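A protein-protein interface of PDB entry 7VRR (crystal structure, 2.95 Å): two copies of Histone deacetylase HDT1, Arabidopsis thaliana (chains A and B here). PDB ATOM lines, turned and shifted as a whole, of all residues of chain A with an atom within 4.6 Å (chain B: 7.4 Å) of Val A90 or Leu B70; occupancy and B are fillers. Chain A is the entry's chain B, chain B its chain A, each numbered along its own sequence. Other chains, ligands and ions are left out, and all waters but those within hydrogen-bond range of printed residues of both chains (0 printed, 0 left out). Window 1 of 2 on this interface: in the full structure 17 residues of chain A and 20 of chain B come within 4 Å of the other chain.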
ATOM      1  N   PHE A   3      -0.582 -32.131 -34.576  1.00  0.00           N
ATOM      2  CA  PHE A   3      -1.062 -31.700 -33.272  1.00  0.00           C
ATOM      3  C   PHE A   3      -1.958 -32.750 -32.617  1.00  0.00           C
ATOM      4  O   PHE A   3      -2.768 -33.390 -33.291  1.00  0.00           O
ATOM      5  CB  PHE A   3      -1.820 -30.367 -33.384  1.00  0.00           C
ATOM      6  CG  PHE A   3      -2.373 -29.885 -32.081  1.00  0.00           C
ATOM      7  CD1 PHE A   3      -3.609 -30.308 -31.646  1.00  0.00           C
ATOM      8  CD2 PHE A   3      -1.641 -29.035 -31.274  1.00  0.00           C
ATOM      9  CE1 PHE A   3      -4.124 -29.886 -30.434  1.00  0.00           C
ATOM     10  CE2 PHE A   3      -2.132 -28.621 -30.048  1.00  0.00           C
ATOM     11  CZ  PHE A   3      -3.379 -29.043 -29.627  1.00  0.00           C
ATOM     12  N   TRP A   4      -1.791 -32.929 -31.302  1.00  0.00           N
ATOM     13  CA  TRP A   4      -2.673 -33.776 -30.514  1.00  0.00           C
ATOM     14  C   TRP A   4      -2.921 -33.110 -29.170  1.00  0.00           C
ATOM     15  O   TRP A   4      -2.025 -32.507 -28.605  1.00  0.00           O
ATOM     16  CB  TRP A   4      -2.063 -35.162 -30.305  1.00  0.00           C
ATOM     17  CG  TRP A   4      -2.892 -36.031 -29.405  1.00  0.00           C
ATOM     18  CD1 TRP A   4      -3.934 -36.816 -29.764  1.00  0.00           C
ATOM     19  CD2 TRP A   4      -2.751 -36.179 -27.985  1.00  0.00           C
ATOM     20  NE1 TRP A   4      -4.457 -37.452 -28.666  1.00  0.00           N
ATOM     21  CE2 TRP A   4      -3.749 -37.075 -27.557  1.00  0.00           C
ATOM     22  CE3 TRP A   4      -1.870 -35.643 -27.033  1.00  0.00           C
ATOM     23  CZ2 TRP A   4      -3.897 -37.451 -26.220  1.00  0.00           C
ATOM     24  CZ3 TRP A   4      -2.019 -36.010 -25.706  1.00  0.00           C
ATOM     25  CH2 TRP A   4      -3.027 -36.904 -25.313  1.00  0.00           C
ATOM     26  N   GLY A   5      -4.139 -33.236 -28.648  1.00  0.00           N
ATOM     27  CA  GLY A   5      -4.449 -32.716 -27.339  1.00  0.00           C
ATOM     28  C   GLY A   5      -5.801 -33.189 -26.874  1.00  0.00           C
ATOM     29  O   GLY A   5      -6.685 -33.419 -27.690  1.00  0.00           O
ATOM     30  N   VAL A  26       3.091 -37.167 -25.605  1.00  0.00           N
ATOM     31  CA  VAL A  26       2.567 -36.181 -24.670  1.00  0.00           C
ATOM     32  C   VAL A  26       3.708 -35.298 -24.167  1.00  0.00           C
ATOM     33  O   VAL A  26       4.709 -35.799 -23.606  1.00  0.00           O
ATOM     34  CB  VAL A  26       1.872 -36.837 -23.471  1.00  0.00           C
ATOM     35  CG1 VAL A  26       1.295 -35.745 -22.549  1.00  0.00           C
ATOM     36  CG2 VAL A  26       0.782 -37.795 -23.951  1.00  0.00           C
ATOM     37  N   SER A  27       3.540 -33.988 -24.388  1.00  0.00           N
ATOM     38  CA  SER A  27       4.537 -32.971 -24.114  1.00  0.00           C
ATOM     39  C   SER A  27       4.255 -32.202 -22.839  1.00  0.00           C
ATOM     40  O   SER A  27       5.162 -31.601 -22.279  1.00  0.00           O
ATOM     41  CB  SER A  27       4.615 -31.974 -25.266  1.00  0.00           C
ATOM     42  OG  SER A  27       5.234 -32.552 -26.383  1.00  0.00           O
ATOM     43  N   GLN A  28       2.995 -32.189 -22.398  1.00  0.00           N
ATOM     44  CA  GLN A  28       2.631 -31.457 -21.193  1.00  0.00           C
ATOM     45  C   GLN A  28       1.238 -31.700 -20.652  1.00  0.00           C
ATOM     46  O   GLN A  28       0.346 -32.174 -21.368  1.00  0.00           O
ATOM     47  CB  GLN A  28       2.775 -29.964 -21.416  1.00  0.00           C
ATOM     48  CG  GLN A  28       1.906 -29.434 -22.533  1.00  0.00           C
ATOM     49  CD  GLN A  28       2.031 -27.924 -22.634  1.00  0.00           C
ATOM     50  OE1 GLN A  28       3.135 -27.381 -22.774  1.00  0.00           O
ATOM     51  NE2 GLN A  28       0.908 -27.236 -22.545  1.00  0.00           N
ATOM     52  N   TYR A  88      -5.644 -30.489 -19.128  1.00  0.00           N
ATOM     53  CA  TYR A  88      -5.355 -30.583 -20.582  1.00  0.00           C
ATOM     54  C   TYR A  88      -4.010 -31.288 -20.772  1.00  0.00           C
ATOM     55  O   TYR A  88      -3.018 -30.867 -20.134  1.00  0.00           O
ATOM     56  CB  TYR A  88      -5.368 -29.194 -21.220  1.00  0.00           C
ATOM     57  CG  TYR A  88      -6.677 -28.464 -21.083  1.00  0.00           C
ATOM     58  CD1 TYR A  88      -6.953 -27.706 -19.962  1.00  0.00           C
ATOM     59  CD2 TYR A  88      -7.644 -28.525 -22.074  1.00  0.00           C
ATOM     60  CE1 TYR A  88      -8.152 -27.027 -19.827  1.00  0.00           C
ATOM     61  CE2 TYR A  88      -8.850 -27.851 -21.958  1.00  0.00           C
ATOM     62  CZ  TYR A  88      -9.102 -27.099 -20.828  1.00  0.00           C
ATOM     63  OH  TYR A  88     -10.276 -26.419 -20.707  1.00  0.00           O
ATOM     64  N   PHE A  89      -3.996 -32.341 -21.597  1.00  0.00           N
ATOM     65  CA  PHE A  89      -2.774 -33.035 -21.993  1.00  0.00           C
ATOM     66  C   PHE A  89      -2.541 -32.724 -23.459  1.00  0.00           C
ATOM     67  O   PHE A  89      -3.425 -32.934 -24.287  1.00  0.00           O
ATOM     68  CB  PHE A  89      -2.904 -34.543 -21.782  1.00  0.00           C
ATOM     69  CG  PHE A  89      -3.035 -34.940 -20.346  1.00  0.00           C
ATOM     70  CD1 PHE A  89      -4.247 -34.842 -19.699  1.00  0.00           C
ATOM     71  CD2 PHE A  89      -1.944 -35.409 -19.641  1.00  0.00           C
ATOM     72  CE1 PHE A  89      -4.380 -35.198 -18.370  1.00  0.00           C
ATOM     73  CE2 PHE A  89      -2.062 -35.788 -18.315  1.00  0.00           C
ATOM     74  CZ  PHE A  89      -3.281 -35.680 -17.676  1.00  0.00           C
ATOM     75  N   VAL A  90      -1.352 -32.204 -23.779  1.00  0.00           N
ATOM     76  CA  VAL A  90      -1.082 -31.715 -25.125  1.00  0.00           C
ATOM     77  C   VAL A  90       0.238 -32.261 -25.639  1.00  0.00           C
ATOM     78  O   VAL A  90       1.180 -32.439 -24.879  1.00  0.00           O
ATOM     79  CB  VAL A  90      -1.060 -30.177 -25.167  1.00  0.00           C
ATOM     80  CG1 VAL A  90      -0.810 -29.688 -26.588  1.00  0.00           C
ATOM     81  CG2 VAL A  90      -2.370 -29.615 -24.641  1.00  0.00           C
ATOM     82  N   GLY A  91       0.279 -32.539 -26.943  1.00  0.00           N
ATOM     83  CA  GLY A  91       1.466 -33.033 -27.608  1.00  0.00           C
ATOM     84  C   GLY A  91       1.264 -33.134 -29.107  1.00  0.00           C
ATOM     85  O   GLY A  91       0.640 -32.267 -29.744  1.00  0.00           O
ATOM     86  N   LEU B  23       5.614 -27.302 -40.240  1.00  0.00           N
ATOM     87  CA  LEU B  23       5.242 -27.343 -38.839  1.00  0.00           C
ATOM     88  C   LEU B  23       5.746 -26.086 -38.157  1.00  0.00           C
ATOM     89  O   LEU B  23       6.876 -25.650 -38.403  1.00  0.00           O
ATOM     90  CB  LEU B  23       5.904 -28.523 -38.132  1.00  0.00           C
ATOM     91  CG  LEU B  23       5.590 -29.924 -38.617  1.00  0.00           C
ATOM     92  CD1 LEU B  23       6.440 -30.902 -37.812  1.00  0.00           C
ATOM     93  CD2 LEU B  23       4.128 -30.371 -38.413  1.00  0.00           C
ATOM     94  N   ILE B  24       4.925 -25.548 -37.252  1.00  0.00           N
ATOM     95  CA  ILE B  24       5.373 -24.547 -36.297  1.00  0.00           C
ATOM     96  C   ILE B  24       5.553 -25.216 -34.933  1.00  0.00           C
ATOM     97  O   ILE B  24       4.597 -25.705 -34.338  1.00  0.00           O
ATOM     98  CB  ILE B  24       4.391 -23.373 -36.198  1.00  0.00           C
ATOM     99  CG1 ILE B  24       4.162 -22.791 -37.602  1.00  0.00           C
ATOM    100  CG2 ILE B  24       4.881 -22.357 -35.155  1.00  0.00           C
ATOM    101  CD1 ILE B  24       4.797 -21.457 -37.913  1.00  0.00           C
ATOM    102  N   HIS B  25       6.806 -25.253 -34.471  1.00  0.00           N
ATOM    103  CA  HIS B  25       7.166 -25.715 -33.145  1.00  0.00           C
ATOM    104  C   HIS B  25       7.256 -24.514 -32.222  1.00  0.00           C
ATOM    105  O   HIS B  25       8.046 -23.594 -32.474  1.00  0.00           O
ATOM    106  CB  HIS B  25       8.511 -26.445 -33.167  1.00  0.00           C
ATOM    107  CG  HIS B  25       8.858 -27.098 -31.869  1.00  0.00           C
ATOM    108  ND1 HIS B  25       9.439 -26.413 -30.825  1.00  0.00           N
ATOM    109  CD2 HIS B  25       8.706 -28.376 -31.446  1.00  0.00           C
ATOM    110  CE1 HIS B  25       9.626 -27.243 -29.807  1.00  0.00           C
ATOM    111  NE2 HIS B  25       9.205 -28.442 -30.167  1.00  0.00           N
ATOM    112  N   VAL B  26       6.437 -24.537 -31.168  1.00  0.00           N
ATOM    113  CA  VAL B  26       6.497 -23.578 -30.061  1.00  0.00           C
ATOM    114  C   VAL B  26       7.291 -24.178 -28.902  1.00  0.00           C
ATOM    115  O   VAL B  26       6.957 -25.258 -28.384  1.00  0.00           O
ATOM    116  CB  VAL B  26       5.096 -23.179 -29.559  1.00  0.00           C
ATOM    117  CG1 VAL B  26       5.218 -22.138 -28.450  1.00  0.00           C
ATOM    118  CG2 VAL B  26       4.249 -22.669 -30.710  1.00  0.00           C
ATOM    119  N   SER B  27       8.343 -23.454 -28.517  1.00  0.00           N
ATOM    120  CA  SER B  27       9.310 -23.870 -27.518  1.00  0.00           C
ATOM    121  C   SER B  27       9.095 -23.202 -26.177  1.00  0.00           C
ATOM    122  O   SER B  27       9.558 -23.714 -25.157  1.00  0.00           O
ATOM    123  CB  SER B  27      10.734 -23.559 -27.986  1.00  0.00           C
ATOM    124  OG  SER B  27      11.128 -24.433 -29.020  1.00  0.00           O
ATOM    125  N   GLN B  28       8.424 -22.044 -26.171  1.00  0.00           N
ATOM    126  CA  GLN B  28       8.194 -21.324 -24.924  1.00  0.00           C
ATOM    127  C   GLN B  28       7.231 -20.156 -25.000  1.00  0.00           C
ATOM    128  O   GLN B  28       6.963 -19.603 -26.085  1.00  0.00           O
ATOM    129  CB  GLN B  28       9.506 -20.795 -24.365  1.00  0.00           C
ATOM    130  CG  GLN B  28      10.222 -19.861 -25.312  1.00  0.00           C
ATOM    131  CD  GLN B  28      11.430 -19.233 -24.653  1.00  0.00           C
ATOM    132  OE1 GLN B  28      12.311 -19.930 -24.132  1.00  0.00           O
ATOM    133  NE2 GLN B  28      11.478 -17.907 -24.674  1.00  0.00           N
ATOM    134  N   VAL B  46      -5.146 -21.755 -26.486  1.00  0.00           N
ATOM    135  CA  VAL B  46      -4.990 -22.057 -27.894  1.00  0.00           C
ATOM    136  C   VAL B  46      -6.288 -22.640 -28.448  1.00  0.00           C
ATOM    137  O   VAL B  46      -6.993 -23.380 -27.761  1.00  0.00           O
ATOM    138  CB  VAL B  46      -3.797 -23.012 -28.153  1.00  0.00           C
ATOM    139  CG1 VAL B  46      -4.103 -24.418 -27.664  1.00  0.00           C
ATOM    140  CG2 VAL B  46      -3.437 -23.041 -29.635  1.00  0.00           C
ATOM    141  N   LEU B  53      -8.094 -25.204 -25.868  1.00  0.00           N
ATOM    142  CA  LEU B  53      -7.293 -25.820 -24.816  1.00  0.00           C
ATOM    143  C   LEU B  53      -6.479 -24.768 -24.079  1.00  0.00           C
ATOM    144  O   LEU B  53      -6.243 -23.672 -24.590  1.00  0.00           O
ATOM    145  CB  LEU B  53      -6.363 -26.884 -25.408  1.00  0.00           C
ATOM    146  CG  LEU B  53      -7.003 -27.936 -26.326  1.00  0.00           C
ATOM    147  CD1 LEU B  53      -5.941 -28.641 -27.162  1.00  0.00           C
ATOM    148  CD2 LEU B  53      -7.799 -28.942 -25.509  1.00  0.00           C
ATOM    149  N   VAL B  54      -6.049 -25.130 -22.870  1.00  0.00           N
ATOM    150  CA  VAL B  54      -5.225 -24.293 -22.024  1.00  0.00           C
ATOM    151  C   VAL B  54      -3.810 -24.858 -22.008  1.00  0.00           C
ATOM    152  O   VAL B  54      -3.606 -26.002 -21.610  1.00  0.00           O
ATOM    153  CB  VAL B  54      -5.789 -24.236 -20.590  1.00  0.00           C
ATOM    154  CG1 VAL B  54      -4.829 -23.500 -19.667  1.00  0.00           C
ATOM    155  CG2 VAL B  54      -7.157 -23.570 -20.586  1.00  0.00           C
ATOM    156  N   LEU B  55      -2.842 -24.039 -22.441  1.00  0.00           N
ATOM    157  CA  LEU B  55      -1.439 -24.432 -22.557  1.00  0.00           C
ATOM    158  C   LEU B  55      -0.657 -24.266 -21.268  1.00  0.00           C
ATOM    159  O   LEU B  55       0.437 -24.818 -21.123  1.00  0.00           O
ATOM    160  CB  LEU B  55      -0.747 -23.610 -23.645  1.00  0.00           C
ATOM    161  CG  LEU B  55      -1.344 -23.791 -25.038  1.00  0.00           C
ATOM    162  CD1 LEU B  55      -0.523 -22.991 -26.045  1.00  0.00           C
ATOM    163  CD2 LEU B  55      -1.398 -25.270 -25.415  1.00  0.00           C
ATOM    164  N   LEU B  66       7.165 -20.273 -19.274  1.00  0.00           N
ATOM    165  CA  LEU B  66       7.199 -21.721 -19.281  1.00  0.00           C
ATOM    166  C   LEU B  66       7.822 -22.246 -20.554  1.00  0.00           C
ATOM    167  O   LEU B  66       7.769 -21.607 -21.629  1.00  0.00           O
ATOM    168  CB  LEU B  66       5.806 -22.319 -19.076  1.00  0.00           C
ATOM    169  CG  LEU B  66       4.720 -22.158 -20.126  1.00  0.00           C
ATOM    170  CD1 LEU B  66       4.974 -23.002 -21.358  1.00  0.00           C
ATOM    171  CD2 LEU B  66       3.386 -22.533 -19.518  1.00  0.00           C
ATOM    172  N   PHE B  67       8.412 -23.432 -20.418  1.00  0.00           N
ATOM    173  CA  PHE B  67       9.060 -24.142 -21.497  1.00  0.00           C
ATOM    174  C   PHE B  67       8.105 -25.221 -22.032  1.00  0.00           C
ATOM    175  O   PHE B  67       7.345 -25.835 -21.263  1.00  0.00           O
ATOM    176  CB  PHE B  67      10.351 -24.755 -20.967  1.00  0.00           C
ATOM    177  CG  PHE B  67      10.945 -25.742 -21.886  1.00  0.00           C
ATOM    178  CD1 PHE B  67      11.709 -25.324 -22.955  1.00  0.00           C
ATOM    179  CD2 PHE B  67      10.689 -27.089 -21.729  1.00  0.00           C
ATOM    180  CE1 PHE B  67      12.239 -26.236 -23.840  1.00  0.00           C
ATOM    181  CE2 PHE B  67      11.205 -28.003 -22.617  1.00  0.00           C
ATOM    182  CZ  PHE B  67      11.982 -27.580 -23.671  1.00  0.00           C
ATOM    183  N   CYS B  68       8.124 -25.439 -23.356  1.00  0.00           N
ATOM    184  CA  CYS B  68       7.251 -26.433 -23.973  1.00  0.00           C
ATOM    185  C   CYS B  68       7.784 -27.050 -25.261  1.00  0.00           C
ATOM    186  O   CYS B  68       8.713 -26.553 -25.859  1.00  0.00           O
ATOM    187  CB  CYS B  68       5.858 -25.842 -24.191  1.00  0.00           C
ATOM    188  SG  CYS B  68       5.838 -24.279 -25.078  1.00  0.00           S
ATOM    189  N   ASP B  69       7.176 -28.174 -25.646  1.00  0.00           N
ATOM    190  CA  ASP B  69       7.478 -28.908 -26.860  1.00  0.00           C
ATOM    191  C   ASP B  69       6.164 -29.101 -27.613  1.00  0.00           C
ATOM    192  O   ASP B  69       5.602 -30.189 -27.612  1.00  0.00           O
ATOM    193  CB  ASP B  69       8.112 -30.254 -26.490  1.00  0.00           C
ATOM    194  CG  ASP B  69       8.305 -31.179 -27.689  1.00  0.00           C
ATOM    195  OD1 ASP B  69       8.503 -30.689 -28.814  1.00  0.00           O
ATOM    196  OD2 ASP B  69       8.261 -32.414 -27.517  1.00  0.00           O
ATOM    197  N   LEU B  70       5.670 -28.020 -28.227  1.00  0.00           N
ATOM    198  CA  LEU B  70       4.382 -28.031 -28.918  1.00  0.00           C
ATOM    199  C   LEU B  70       4.561 -27.970 -30.434  1.00  0.00           C
ATOM    200  O   LEU B  70       5.339 -27.168 -30.936  1.00  0.00           O
ATOM    201  CB  LEU B  70       3.519 -26.862 -28.454  1.00  0.00           C
ATOM    202  CG  LEU B  70       3.157 -26.858 -26.970  1.00  0.00           C
ATOM    203  CD1 LEU B  70       2.363 -25.621 -26.587  1.00  0.00           C
ATOM    204  CD2 LEU B  70       2.365 -28.102 -26.598  1.00  0.00           C
ATOM    205  N   VAL B  71       3.845 -28.838 -31.150  1.00  0.00           N
ATOM    206  CA  VAL B  71       3.920 -28.903 -32.603  1.00  0.00           C
ATOM    207  C   VAL B  71       2.546 -28.593 -33.197  1.00  0.00           C
ATOM    208  O   VAL B  71       1.544 -29.180 -32.793  1.00  0.00           O
ATOM    209  CB  VAL B  71       4.392 -30.291 -33.089  1.00  0.00           C
ATOM    210  CG1 VAL B  71       4.172 -30.440 -34.588  1.00  0.00           C
ATOM    211  CG2 VAL B  71       5.851 -30.511 -32.748  1.00  0.00           C
ATOM    212  N   PHE B  72       2.510 -27.650 -34.145  1.00  0.00           N
ATOM    213  CA  PHE B  72       1.293 -27.288 -34.859  1.00  0.00           C
ATOM    214  C   PHE B  72       1.467 -27.511 -36.367  1.00  0.00           C
ATOM    215  O   PHE B  72       2.330 -26.895 -37.000  1.00  0.00           O
ATOM    216  CB  PHE B  72       0.901 -25.840 -34.560  1.00  0.00           C
ATOM    217  CG  PHE B  72       0.560 -25.599 -33.122  1.00  0.00           C
ATOM    218  CD1 PHE B  72      -0.717 -25.876 -32.654  1.00  0.00           C
ATOM    219  CD2 PHE B  72       1.508 -25.109 -32.231  1.00  0.00           C
ATOM    220  CE1 PHE B  72      -1.048 -25.656 -31.325  1.00  0.00           C
ATOM    221  CE2 PHE B  72       1.187 -24.902 -30.908  1.00  0.00           C
ATOM    222  CZ  PHE B  72      -0.092 -25.174 -30.450  1.00  0.00           C
ATOM    223  N   LEU B  78      -3.561 -18.304 -30.779  1.00  0.00           N
ATOM    224  CA  LEU B  78      -3.040 -18.108 -29.417  1.00  0.00           C
ATOM    225  C   LEU B  78      -3.673 -16.862 -28.817  1.00  0.00           C
ATOM    226  O   LEU B  78      -3.921 -15.889 -29.537  1.00  0.00           O
ATOM    227  CB  LEU B  78      -1.513 -17.980 -29.429  1.00  0.00           C
ATOM    228  CG  LEU B  78      -0.758 -19.229 -29.909  1.00  0.00           C
ATOM    229  CD1 LEU B  78       0.696 -18.922 -30.164  1.00  0.00           C
ATOM    230  CD2 LEU B  78      -0.891 -20.344 -28.881  1.00  0.00           C
ATOM    231  N   PHE B  89       5.433 -15.817 -27.630  1.00  0.00           N
ATOM    232  CA  PHE B  89       5.554 -17.241 -27.931  1.00  0.00           C
ATOM    233  C   PHE B  89       6.688 -17.399 -28.929  1.00  0.00           C
ATOM    234  O   PHE B  89       6.673 -16.765 -29.972  1.00  0.00           O
ATOM    235  CB  PHE B  89       4.257 -17.805 -28.508  1.00  0.00           C
ATOM    236  CG  PHE B  89       3.105 -17.766 -27.555  1.00  0.00           C
ATOM    237  CD1 PHE B  89       2.393 -16.592 -27.358  1.00  0.00           C
ATOM    238  CD2 PHE B  89       2.736 -18.900 -26.856  1.00  0.00           C
ATOM    239  CE1 PHE B  89       1.320 -16.561 -26.483  1.00  0.00           C
ATOM    240  CE2 PHE B  89       1.673 -18.875 -25.972  1.00  0.00           C
ATOM    241  CZ  PHE B  89       0.952 -17.706 -25.793  1.00  0.00           C
ATOM    242  N   TYR B  92      10.464 -22.339 -33.563  1.00  0.00           N
ATOM    243  CA  TYR B  92      11.027 -22.465 -34.935  1.00  0.00           C
ATOM    244  C   TYR B  92      10.016 -23.142 -35.863  1.00  0.00           C
ATOM    245  O   TYR B  92       9.113 -23.822 -35.362  1.00  0.00           O
ATOM    246  CB  TYR B  92      12.352 -23.232 -34.923  1.00  0.00           C
ATOM    247  CG  TYR B  92      12.355 -24.436 -34.018  1.00  0.00           C
ATOM    248  CD1 TYR B  92      12.722 -24.317 -32.689  1.00  0.00           C
ATOM    249  CD2 TYR B  92      11.977 -25.691 -34.475  1.00  0.00           C
ATOM    250  CE1 TYR B  92      12.722 -25.413 -31.839  1.00  0.00           C
ATOM    251  CE2 TYR B  92      11.979 -26.797 -33.643  1.00  0.00           C
ATOM    252  CZ  TYR B  92      12.336 -26.654 -32.314  1.00  0.00           C
ATOM    253  OH  TYR B  92      12.324 -27.734 -31.478  1.00  0.00           O
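The backbone carbonyl oxygen (O) of Leu B55 sits at hydrogen-bond distance from the side-chain amide nitrogen (NE2) of Gln A28 (2.8 Å).
The side-chain hydroxyl (OG) of Ser A27 is in hydrogen-bond range of the backbone carbonyl oxygen (O) of Asp B69.
Positions printed for both chains: 26, 27, 28 and 89.
Of the 20 printed residues of chain B, 8 touch a printed residue of chain A.
Hydrophobic or aromatic side chains of chain B within 4 Å of the printed part of chain A: Leu B53, Val B54, Leu B70 and Phe B72.
Printed residues of chain A that touch a printed residue of chain B: Phe A3, Ser A27, Gln A28, Tyr A88 and Val A90.
Among the printed residues, pairs that only touch across the chains: Phe A3 with Phe B72, Gln A28 with Cys B68, Tyr A88 with Leu B53, Phe A3 with Val B71, Val A90 with Leu B70, Phe A3 with Leu B53, Tyr A88 with Val B54 and Gln A28 with Leu B70.
The backbone carbonyl oxygen (O) of Ile B24 is in hydrogen-bond range of the backbone NH (N) of Phe B72 (2.9 Å).
NE2 of His B25 is in hydrogen-bond range of OD1 of Asp B69 (2.7 Å).
The backbone NH of Val B26 sits at hydrogen-bond distance from the backbone carbonyl oxygen of Leu B70.
The side-chain sulfur (SG) of Cys B68 lies within hydrogen-bond range of the backbone NH (N) of Gln B28.
N of Leu B53 lies within hydrogen-bond range of O of Val B46 (2.9 Å).
O of Val A90 is in hydrogen-bond range of N of Ser A27 (2.9 Å).
Printed residues of chain B within 4 Å of Gln A28: Leu B55, Cys B68 and Leu B70.
Val A90 touches just one residue of chain B: Leu B70 (3.5 Å).
Val B26 touches none of the printed residues of chain A.
Phe B67 touches none of the printed residues of chain A.
Of the printed residues of chain A, Asp B69 touches Ser A27 (2.7 Å).
The nearest residue of chain B that does not touch Val A90 is Leu B53 (4.5 Å).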
